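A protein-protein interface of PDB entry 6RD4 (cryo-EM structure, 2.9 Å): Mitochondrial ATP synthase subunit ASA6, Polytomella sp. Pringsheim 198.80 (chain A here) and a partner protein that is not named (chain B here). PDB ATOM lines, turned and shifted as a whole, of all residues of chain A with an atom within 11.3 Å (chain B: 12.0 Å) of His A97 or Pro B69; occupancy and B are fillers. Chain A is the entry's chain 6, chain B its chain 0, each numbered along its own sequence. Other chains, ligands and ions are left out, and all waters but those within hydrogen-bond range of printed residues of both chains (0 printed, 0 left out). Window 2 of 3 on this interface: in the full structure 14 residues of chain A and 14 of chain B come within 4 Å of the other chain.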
ATOM      1  N   ARG A  89      -1.833   1.150   0.865  1.00  0.00           N
ATOM      2  CA  ARG A  89      -2.229   1.916   2.028  1.00  0.00           C
ATOM      3  C   ARG A  89      -3.112   1.112   2.951  1.00  0.00           C
ATOM      4  O   ARG A  89      -3.054   1.311   4.158  1.00  0.00           O
ATOM      5  CB  ARG A  89      -2.953   3.176   1.604  1.00  0.00           C
ATOM      6  CG  ARG A  89      -2.073   4.199   1.011  1.00  0.00           C
ATOM      7  CD  ARG A  89      -1.231   4.844   2.023  1.00  0.00           C
ATOM      8  NE  ARG A  89      -2.038   5.344   3.111  1.00  0.00           N
ATOM      9  CZ  ARG A  89      -1.620   6.254   3.970  1.00  0.00           C
ATOM     10  NH1 ARG A  89      -0.412   6.766   3.850  1.00  0.00           N
ATOM     11  NH2 ARG A  89      -2.408   6.649   4.946  1.00  0.00           N
ATOM     12  N   ALA A  90      -3.933   0.212   2.417  1.00  0.00           N
ATOM     13  CA  ALA A  90      -4.717  -0.677   3.260  1.00  0.00           C
ATOM     14  C   ALA A  90      -3.891  -1.799   3.838  1.00  0.00           C
ATOM     15  O   ALA A  90      -4.311  -2.417   4.813  1.00  0.00           O
ATOM     16  CB  ALA A  90      -5.874  -1.282   2.483  1.00  0.00           C
ATOM     17  N   ASP A  91      -2.746  -2.096   3.238  1.00  0.00           N
ATOM     18  CA  ASP A  91      -1.848  -3.085   3.803  1.00  0.00           C
ATOM     19  C   ASP A  91      -1.214  -2.569   5.076  1.00  0.00           C
ATOM     20  O   ASP A  91      -1.247  -3.237   6.110  1.00  0.00           O
ATOM     21  CB  ASP A  91      -0.781  -3.451   2.784  1.00  0.00           C
ATOM     22  CG  ASP A  91       0.389  -4.164   3.399  1.00  0.00           C
ATOM     23  OD1 ASP A  91       0.236  -5.335   3.808  1.00  0.00           O
ATOM     24  OD2 ASP A  91       1.473  -3.552   3.474  1.00  0.00           O
ATOM     25  N   GLY A  92      -0.648  -1.367   5.027  1.00  0.00           N
ATOM     26  CA  GLY A  92      -0.025  -0.783   6.194  1.00  0.00           C
ATOM     27  C   GLY A  92      -0.989  -0.184   7.180  1.00  0.00           C
ATOM     28  O   GLY A  92      -0.581   0.164   8.287  1.00  0.00           O
ATOM     29  N   GLN A  93      -2.243  -0.006   6.790  1.00  0.00           N
ATOM     30  CA  GLN A  93      -3.278   0.364   7.742  1.00  0.00           C
ATOM     31  C   GLN A  93      -3.690  -0.804   8.593  1.00  0.00           C
ATOM     32  O   GLN A  93      -4.165  -0.605   9.710  1.00  0.00           O
ATOM     33  CB  GLN A  93      -4.522   0.871   7.037  1.00  0.00           C
ATOM     34  CG  GLN A  93      -4.624   2.341   6.858  1.00  0.00           C
ATOM     35  CD  GLN A  93      -5.941   2.713   6.276  1.00  0.00           C
ATOM     36  OE1 GLN A  93      -6.700   1.856   5.855  1.00  0.00           O
ATOM     37  NE2 GLN A  93      -6.230   3.995   6.244  1.00  0.00           N
ATOM     38  N   SER A  94      -3.549  -2.013   8.083  1.00  0.00           N
ATOM     39  CA  SER A  94      -3.993  -3.196   8.787  1.00  0.00           C
ATOM     40  C   SER A  94      -2.971  -3.712   9.772  1.00  0.00           C
ATOM     41  O   SER A  94      -3.254  -4.683  10.464  1.00  0.00           O
ATOM     42  CB  SER A  94      -4.314  -4.285   7.791  1.00  0.00           C
ATOM     43  OG  SER A  94      -3.136  -4.672   7.124  1.00  0.00           O
ATOM     44  N   LYS A  95      -1.811  -3.090   9.870  1.00  0.00           N
ATOM     45  CA  LYS A  95      -0.830  -3.453  10.872  1.00  0.00           C
ATOM     46  C   LYS A  95      -0.337  -2.224  11.610  1.00  0.00           C
ATOM     47  O   LYS A  95       0.848  -2.087  11.902  1.00  0.00           O
ATOM     48  CB  LYS A  95       0.324  -4.202  10.234  1.00  0.00           C
ATOM     49  CG  LYS A  95       0.860  -3.554   9.023  1.00  0.00           C
ATOM     50  CD  LYS A  95       1.911  -4.391   8.359  1.00  0.00           C
ATOM     51  CE  LYS A  95       1.300  -5.436   7.473  1.00  0.00           C
ATOM     52  NZ  LYS A  95       2.321  -5.909   6.528  1.00  0.00           N
ATOM     53  N   ALA A  96      -1.243  -1.321  11.966  1.00  0.00           N
ATOM     54  CA  ALA A  96      -0.853   0.017  12.376  1.00  0.00           C
ATOM     55  C   ALA A  96      -0.984   0.258  13.867  1.00  0.00           C
ATOM     56  O   ALA A  96      -0.879   1.413  14.291  1.00  0.00           O
ATOM     57  CB  ALA A  96      -1.686   1.051  11.628  1.00  0.00           C
ATOM     58  N   HIS A  97      -1.265  -0.787  14.647  1.00  0.00           N
ATOM     59  CA  HIS A  97      -1.521  -0.836  16.091  1.00  0.00           C
ATOM     60  C   HIS A  97      -2.871  -0.246  16.472  1.00  0.00           C
ATOM     61  O   HIS A  97      -3.397  -0.535  17.543  1.00  0.00           O
ATOM     62  CB  HIS A  97      -0.409  -0.161  16.910  1.00  0.00           C
ATOM     63  CG  HIS A  97      -0.557  -0.348  18.385  1.00  0.00           C
ATOM     64  ND1 HIS A  97      -0.208  -1.516  19.024  1.00  0.00           N
ATOM     65  CD2 HIS A  97      -1.084   0.459  19.333  1.00  0.00           C
ATOM     66  CE1 HIS A  97      -0.483  -1.407  20.308  1.00  0.00           C
ATOM     67  NE2 HIS A  97      -1.019  -0.220  20.522  1.00  0.00           N
ATOM     68  N   GLU A  98      -3.497   0.491  15.581  1.00  0.00           N
ATOM     69  CA  GLU A  98      -4.867   0.937  15.731  1.00  0.00           C
ATOM     70  C   GLU A  98      -5.627   0.526  14.506  1.00  0.00           C
ATOM     71  O   GLU A  98      -6.413   1.283  13.945  1.00  0.00           O
ATOM     72  CB  GLU A  98      -4.932   2.441  15.931  1.00  0.00           C
ATOM     73  CG  GLU A  98      -4.200   2.942  17.149  1.00  0.00           C
ATOM     74  CD  GLU A  98      -5.071   2.979  18.385  1.00  0.00           C
ATOM     75  OE1 GLU A  98      -6.291   2.752  18.260  1.00  0.00           O
ATOM     76  OE2 GLU A  98      -4.540   3.232  19.484  1.00  0.00           O
ATOM     77  N   TRP A  99      -5.373  -0.711  14.085  1.00  0.00           N
ATOM     78  CA  TRP A  99      -5.695  -1.161  12.739  1.00  0.00           C
ATOM     79  C   TRP A  99      -7.190  -1.214  12.512  1.00  0.00           C
ATOM     80  O   TRP A  99      -7.660  -0.945  11.411  1.00  0.00           O
ATOM     81  CB  TRP A  99      -5.075  -2.533  12.493  1.00  0.00           C
ATOM     82  CG  TRP A  99      -5.492  -3.534  13.490  1.00  0.00           C
ATOM     83  CD1 TRP A  99      -4.917  -3.774  14.682  1.00  0.00           C
ATOM     84  CD2 TRP A  99      -6.600  -4.417  13.395  1.00  0.00           C
ATOM     85  NE1 TRP A  99      -5.595  -4.753  15.346  1.00  0.00           N
ATOM     86  CE2 TRP A  99      -6.640  -5.160  14.569  1.00  0.00           C
ATOM     87  CE3 TRP A  99      -7.575  -4.641  12.430  1.00  0.00           C
ATOM     88  CZ2 TRP A  99      -7.599  -6.109  14.801  1.00  0.00           C
ATOM     89  CZ3 TRP A  99      -8.520  -5.575  12.667  1.00  0.00           C
ATOM     90  CH2 TRP A  99      -8.531  -6.303  13.836  1.00  0.00           C
ATOM     91  N   ILE A 100      -7.958  -1.554  13.540  1.00  0.00           N
ATOM     92  CA  ILE A 100      -9.396  -1.608  13.377  1.00  0.00           C
ATOM     93  C   ILE A 100      -9.976  -0.211  13.432  1.00  0.00           C
ATOM     94  O   ILE A 100     -11.025   0.045  12.845  1.00  0.00           O
ATOM     95  CB  ILE A 100      -9.993  -2.571  14.421  1.00  0.00           C
ATOM     96  CG1 ILE A 100     -11.460  -2.872  14.148  1.00  0.00           C
ATOM     97  CG2 ILE A 100      -9.812  -2.053  15.801  1.00  0.00           C
ATOM     98  CD1 ILE A 100     -11.709  -3.467  12.817  1.00  0.00           C
ATOM     99  N   VAL A 101      -9.290   0.729  14.065  1.00  0.00           N
ATOM    100  CA  VAL A 101      -9.755   2.103  14.024  1.00  0.00           C
ATOM    101  C   VAL A 101      -9.372   2.744  12.698  1.00  0.00           C
ATOM    102  O   VAL A 101     -10.130   3.541  12.145  1.00  0.00           O
ATOM    103  CB  VAL A 101      -9.206   2.868  15.235  1.00  0.00           C
ATOM    104  CG1 VAL A 101      -9.740   4.259  15.268  1.00  0.00           C
ATOM    105  CG2 VAL A 101      -9.574   2.144  16.496  1.00  0.00           C
ATOM    106  N   ASP A 102      -8.212   2.379  12.150  1.00  0.00           N
ATOM    107  CA  ASP A 102      -7.807   2.894  10.847  1.00  0.00           C
ATOM    108  C   ASP A 102      -8.703   2.367   9.746  1.00  0.00           C
ATOM    109  O   ASP A 102      -9.087   3.115   8.850  1.00  0.00           O
ATOM    110  CB  ASP A 102      -6.367   2.514  10.531  1.00  0.00           C
ATOM    111  CG  ASP A 102      -5.376   3.228  11.393  1.00  0.00           C
ATOM    112  OD1 ASP A 102      -5.794   3.801  12.401  1.00  0.00           O
ATOM    113  OD2 ASP A 102      -4.176   3.216  11.066  1.00  0.00           O
ATOM    114  N   LEU A 103      -9.051   1.089   9.792  1.00  0.00           N
ATOM    115  CA  LEU A 103      -9.900   0.526   8.760  1.00  0.00           C
ATOM    116  C   LEU A 103     -11.351   0.930   8.920  1.00  0.00           C
ATOM    117  O   LEU A 103     -12.108   0.843   7.956  1.00  0.00           O
ATOM    118  CB  LEU A 103      -9.787  -0.988   8.758  1.00  0.00           C
ATOM    119  CG  LEU A 103      -8.448  -1.533   8.290  1.00  0.00           C
ATOM    120  CD1 LEU A 103      -8.396  -2.962   8.673  1.00  0.00           C
ATOM    121  CD2 LEU A 103      -8.245  -1.376   6.818  1.00  0.00           C
ATOM    122  N   ASN A 104     -11.768   1.352  10.101  1.00  0.00           N
ATOM    123  CA  ASN A 104     -13.098   1.914  10.245  1.00  0.00           C
ATOM    124  C   ASN A 104     -13.143   3.408  10.012  1.00  0.00           C
ATOM    125  O   ASN A 104     -14.225   3.985  10.076  1.00  0.00           O
ATOM    126  CB  ASN A 104     -13.689   1.610  11.618  1.00  0.00           C
ATOM    127  CG  ASN A 104     -14.212   0.204  11.715  1.00  0.00           C
ATOM    128  OD1 ASN A 104     -13.768  -0.591  12.530  1.00  0.00           O
ATOM    129  ND2 ASN A 104     -15.164  -0.117  10.861  1.00  0.00           N
ATOM    130  N   PRO B  58      11.903  -7.992  15.160  1.00  0.00           N
ATOM    131  CA  PRO B  58      10.468  -8.231  15.305  1.00  0.00           C
ATOM    132  C   PRO B  58       9.642  -6.977  15.147  1.00  0.00           C
ATOM    133  O   PRO B  58       8.481  -7.070  14.742  1.00  0.00           O
ATOM    134  CB  PRO B  58      10.348  -8.808  16.716  1.00  0.00           C
ATOM    135  CG  PRO B  58      11.693  -9.264  17.045  1.00  0.00           C
ATOM    136  CD  PRO B  58      12.625  -8.330  16.387  1.00  0.00           C
ATOM    137  N   ASP B  59      10.203  -5.806  15.444  1.00  0.00           N
ATOM    138  CA  ASP B  59       9.436  -4.570  15.366  1.00  0.00           C
ATOM    139  C   ASP B  59       9.099  -4.201  13.935  1.00  0.00           C
ATOM    140  O   ASP B  59       8.085  -3.544  13.691  1.00  0.00           O
ATOM    141  CB  ASP B  59      10.203  -3.428  16.017  1.00  0.00           C
ATOM    142  CG  ASP B  59       9.891  -3.276  17.481  1.00  0.00           C
ATOM    143  OD1 ASP B  59       8.785  -3.674  17.894  1.00  0.00           O
ATOM    144  OD2 ASP B  59      10.743  -2.747  18.220  1.00  0.00           O
ATOM    145  N   GLN B  60       9.917  -4.617  12.987  1.00  0.00           N
ATOM    146  CA  GLN B  60       9.736  -4.250  11.599  1.00  0.00           C
ATOM    147  C   GLN B  60       8.810  -5.176  10.845  1.00  0.00           C
ATOM    148  O   GLN B  60       8.568  -4.944   9.661  1.00  0.00           O
ATOM    149  CB  GLN B  60      11.077  -4.213  10.903  1.00  0.00           C
ATOM    150  CG  GLN B  60      12.088  -3.457  11.668  1.00  0.00           C
ATOM    151  CD  GLN B  60      11.696  -2.035  11.847  1.00  0.00           C
ATOM    152  OE1 GLN B  60      11.745  -1.502  12.941  1.00  0.00           O
ATOM    153  NE2 GLN B  60      11.302  -1.397  10.764  1.00  0.00           N
ATOM    154  N   HIS B  61       8.278  -6.204  11.480  1.00  0.00           N
ATOM    155  CA  HIS B  61       7.325  -7.104  10.839  1.00  0.00           C
ATOM    156  C   HIS B  61       6.109  -7.270  11.728  1.00  0.00           C
ATOM    157  O   HIS B  61       5.947  -8.313  12.363  1.00  0.00           O
ATOM    158  CB  HIS B  61       7.950  -8.464  10.556  1.00  0.00           C
ATOM    159  CG  HIS B  61       9.175  -8.398   9.713  1.00  0.00           C
ATOM    160  ND1 HIS B  61       9.181  -8.752   8.386  1.00  0.00           N
ATOM    161  CD2 HIS B  61      10.438  -8.017  10.008  1.00  0.00           C
ATOM    162  CE1 HIS B  61      10.394  -8.583   7.897  1.00  0.00           C
ATOM    163  NE2 HIS B  61      11.175  -8.135   8.861  1.00  0.00           N
ATOM    164  N   PRO B  62       5.229  -6.282  11.791  1.00  0.00           N
ATOM    165  CA  PRO B  62       4.008  -6.452  12.567  1.00  0.00           C
ATOM    166  C   PRO B  62       3.009  -7.324  11.833  1.00  0.00           C
ATOM    167  O   PRO B  62       3.053  -7.483  10.619  1.00  0.00           O
ATOM    168  CB  PRO B  62       3.490  -5.028  12.716  1.00  0.00           C
ATOM    169  CG  PRO B  62       3.993  -4.349  11.561  1.00  0.00           C
ATOM    170  CD  PRO B  62       5.294  -4.935  11.212  1.00  0.00           C
ATOM    171  N   THR B  63       2.119  -7.914  12.615  1.00  0.00           N
ATOM    172  CA  THR B  63       1.186  -8.895  12.092  1.00  0.00           C
ATOM    173  C   THR B  63       0.093  -8.198  11.306  1.00  0.00           C
ATOM    174  O   THR B  63      -0.438  -7.173  11.725  1.00  0.00           O
ATOM    175  CB  THR B  63       0.622  -9.722  13.242  1.00  0.00           C
ATOM    176  OG1 THR B  63       1.671 -10.533  13.764  1.00  0.00           O
ATOM    177  CG2 THR B  63      -0.494 -10.632  12.813  1.00  0.00           C
ATOM    178  N   ALA B  64      -0.244  -8.778  10.155  1.00  0.00           N
ATOM    179  CA  ALA B  64      -1.053  -8.131   9.144  1.00  0.00           C
ATOM    180  C   ALA B  64      -2.476  -7.845   9.574  1.00  0.00           C
ATOM    181  O   ALA B  64      -3.129  -7.058   8.907  1.00  0.00           O
ATOM    182  CB  ALA B  64      -1.083  -8.992   7.888  1.00  0.00           C
ATOM    183  N   PHE B  65      -2.977  -8.451  10.622  1.00  0.00           N
ATOM    184  CA  PHE B  65      -4.323  -8.166  11.107  1.00  0.00           C
ATOM    185  C   PHE B  65      -4.415  -8.625  12.548  1.00  0.00           C
ATOM    186  O   PHE B  65      -5.217  -9.519  12.842  1.00  0.00           O
ATOM    187  CB  PHE B  65      -5.383  -8.914  10.303  1.00  0.00           C
ATOM    188  CG  PHE B  65      -6.028  -8.114   9.231  1.00  0.00           C
ATOM    189  CD1 PHE B  65      -6.943  -7.151   9.548  1.00  0.00           C
ATOM    190  CD2 PHE B  65      -5.763  -8.366   7.904  1.00  0.00           C
ATOM    191  CE1 PHE B  65      -7.552  -6.431   8.568  1.00  0.00           C
ATOM    192  CE2 PHE B  65      -6.359  -7.636   6.926  1.00  0.00           C
ATOM    193  CZ  PHE B  65      -7.256  -6.671   7.259  1.00  0.00           C
ATOM    194  N   PRO B  66      -3.673  -8.013  13.467  1.00  0.00           N
ATOM    195  CA  PRO B  66      -3.237  -8.732  14.668  1.00  0.00           C
ATOM    196  C   PRO B  66      -4.368  -8.992  15.644  1.00  0.00           C
ATOM    197  O   PRO B  66      -5.194  -8.122  15.909  1.00  0.00           O
ATOM    198  CB  PRO B  66      -2.183  -7.801  15.267  1.00  0.00           C
ATOM    199  CG  PRO B  66      -2.550  -6.486  14.801  1.00  0.00           C
ATOM    200  CD  PRO B  66      -3.208  -6.624  13.471  1.00  0.00           C
ATOM    201  N   LYS B  67      -4.413 -10.225  16.146  1.00  0.00           N
ATOM    202  CA  LYS B  67      -5.442 -10.606  17.094  1.00  0.00           C
ATOM    203  C   LYS B  67      -5.175 -10.025  18.464  1.00  0.00           C
ATOM    204  O   LYS B  67      -6.106  -9.819  19.241  1.00  0.00           O
ATOM    205  CB  LYS B  67      -5.537 -12.118  17.174  1.00  0.00           C
ATOM    206  CG  LYS B  67      -5.848 -12.783  15.863  1.00  0.00           C
ATOM    207  CD  LYS B  67      -7.208 -12.381  15.399  1.00  0.00           C
ATOM    208  CE  LYS B  67      -7.734 -13.304  14.348  1.00  0.00           C
ATOM    209  NZ  LYS B  67      -9.158 -13.005  14.085  1.00  0.00           N
ATOM    210  N   VAL B  68      -3.912  -9.782  18.792  1.00  0.00           N
ATOM    211  CA  VAL B  68      -3.527  -9.067  19.999  1.00  0.00           C
ATOM    212  C   VAL B  68      -2.635  -7.913  19.568  1.00  0.00           C
ATOM    213  O   VAL B  68      -1.721  -8.121  18.771  1.00  0.00           O
ATOM    214  CB  VAL B  68      -2.797  -9.969  21.009  1.00  0.00           C
ATOM    215  CG1 VAL B  68      -2.368  -9.189  22.206  1.00  0.00           C
ATOM    216  CG2 VAL B  68      -3.702 -11.074  21.441  1.00  0.00           C
ATOM    217  N   PRO B  69      -2.888  -6.692  20.025  1.00  0.00           N
ATOM    218  CA  PRO B  69      -2.056  -5.555  19.632  1.00  0.00           C
ATOM    219  C   PRO B  69      -0.610  -5.667  20.061  1.00  0.00           C
ATOM    220  O   PRO B  69      -0.288  -5.599  21.245  1.00  0.00           O
ATOM    221  CB  PRO B  69      -2.743  -4.385  20.333  1.00  0.00           C
ATOM    222  CG  PRO B  69      -4.116  -4.823  20.510  1.00  0.00           C
ATOM    223  CD  PRO B  69      -4.068  -6.256  20.774  1.00  0.00           C
ATOM    224  N   GLY B  70       0.269  -5.824  19.083  1.00  0.00           N
ATOM    225  CA  GLY B  70       1.679  -6.021  19.333  1.00  0.00           C
ATOM    226  C   GLY B  70       2.213  -7.314  18.787  1.00  0.00           C
ATOM    227  O   GLY B  70       3.395  -7.609  18.997  1.00  0.00           O
ATOM    228  N   MET B  71       1.389  -8.108  18.112  1.00  0.00           N
ATOM    229  CA  MET B  71       1.844  -9.350  17.515  1.00  0.00           C
ATOM    230  C   MET B  71       2.761  -9.052  16.349  1.00  0.00           C
ATOM    231  O   MET B  71       2.468  -8.186  15.529  1.00  0.00           O
ATOM    232  CB  MET B  71       0.664 -10.166  17.028  1.00  0.00           C
ATOM    233  CG  MET B  71      -0.041 -10.933  18.082  1.00  0.00           C
ATOM    234  SD  MET B  71      -1.331 -11.930  17.359  1.00  0.00           S
ATOM    235  CE  MET B  71      -0.435 -12.660  16.002  1.00  0.00           C
ATOM    236  N   LYS B  72       3.876  -9.756  16.287  1.00  0.00           N
ATOM    237  CA  LYS B  72       4.840  -9.601  15.218  1.00  0.00           C
ATOM    238  C   LYS B  72       4.954 -10.911  14.465  1.00  0.00           C
ATOM    239  O   LYS B  72       4.633 -11.977  14.983  1.00  0.00           O
ATOM    240  CB  LYS B  72       6.198  -9.175  15.761  1.00  0.00           C
ATOM    241  CG  LYS B  72       6.118  -8.058  16.768  1.00  0.00           C
ATOM    242  CD  LYS B  72       5.535  -6.813  16.158  1.00  0.00           C
ATOM    243  CE  LYS B  72       5.568  -5.653  17.120  1.00  0.00           C
ATOM    244  NZ  LYS B  72       5.050  -4.413  16.501  1.00  0.00           N
ATOM    245  N   ASP B  73       5.397 -10.826  13.221  1.00  0.00           N
ATOM    246  CA  ASP B  73       5.428 -12.014  12.388  1.00  0.00           C
ATOM    247  C   ASP B  73       6.712 -12.802  12.528  1.00  0.00           C
ATOM    248  O   ASP B  73       6.682 -14.032  12.484  1.00  0.00           O
ATOM    249  CB  ASP B  73       5.222 -11.640  10.925  1.00  0.00           C
ATOM    250  CG  ASP B  73       3.775 -11.507  10.572  1.00  0.00           C
ATOM    251  OD1 ASP B  73       2.931 -11.729  11.463  1.00  0.00           O
ATOM    252  OD2 ASP B  73       3.473 -11.189   9.408  1.00  0.00           O
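Among the printed residues, merely in contact across the chains: Lys A95 with Thr B63 (3.4 Å), Leu A103 with Phe B65 (3.6 Å), Ser A94 with Pro B66 (3.6 Å), Ser A94 with Phe B65 (3.7 Å), His A97 with Pro B69 (3.7 Å), Lys A95 with Pro B62 (3.8 Å), Trp A99 with Phe B65 (3.8 Å), Lys A95 with Ala B64 (3.9 Å) and Ser A94 with Thr B63 (3.96 Å).
Printed residues of chain B within 4 Å of His A97: Pro B69 (3.7 Å).
Of chain A, only His A97 (3.7 Å) comes within 4 Å of Pro B69.
No residue of chain B comes within 4 Å of Ala A96.
Pro B66 touches two residues of chain A.
No residue of chain A comes within 4 Å of Val B68.
No residue of chain A comes within 4 Å of Gly B70.
Printed residues of chain A within 4 Å of Phe B65: Ser A94, Trp A99 and Leu A103.
Printed residues of chain B within 4 Å of Leu A103: Phe B65 (3.6 Å).
Of the printed residues of chain A, Pro B62 touches Lys A95 (3.8 Å).
Of the printed residues of chain A, Thr B63 touches Ser A94 and Lys A95.
Of the printed residues of chain B, Ser A94 touches Thr B63 (3.96 Å), Ala B64 (2.8 Å), Phe B65 (3.7 Å) and Pro B66 (3.6 Å).
The nearest residue of chain A that does not touch Pro B69 is Trp A99 (5.4 Å).
Hydrophobic or aromatic side chains of chain A that line the printed part of chain B: His A97, Trp A99 and Leu A103.
Hydrophobic or aromatic side chains of chain B within 4 Å of the printed part of chain A: Pro B62, Phe B65, Pro B66 and Pro B69.
Among the printed residues, 11 pairs touch across the chains.
The side-chain hydroxyl (OG) of Ser A94 is in hydrogen-bond range of the backbone carbonyl oxygen (O) of Ala B64 (3.0 Å).
NE1 of Trp A99 lies close to O of Pro B66 (3.4 Å).
O of Met B71 lies within hydrogen-bond range of N of Thr B63.
N of Lys B72 sits close to OG1 of Thr B63 (3.4 Å).
The side-chain carboxylate (OD1) of Asp B73 lies within hydrogen-bond range of the side-chain hydroxyl (OG1) of Thr B63 (2.9 Å).
The side-chain hydroxyl of Ser A94 is in hydrogen-bond range of the backbone carbonyl oxygen of Ala A90 (3.4 Å).
OG of Ser A94 sits at hydrogen-bond distance from O of Asp A91, 2.6 Å away.
NZ of Lys A95 is in salt-bridge range of OD1 of Asp A91, at 3.5 Å.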
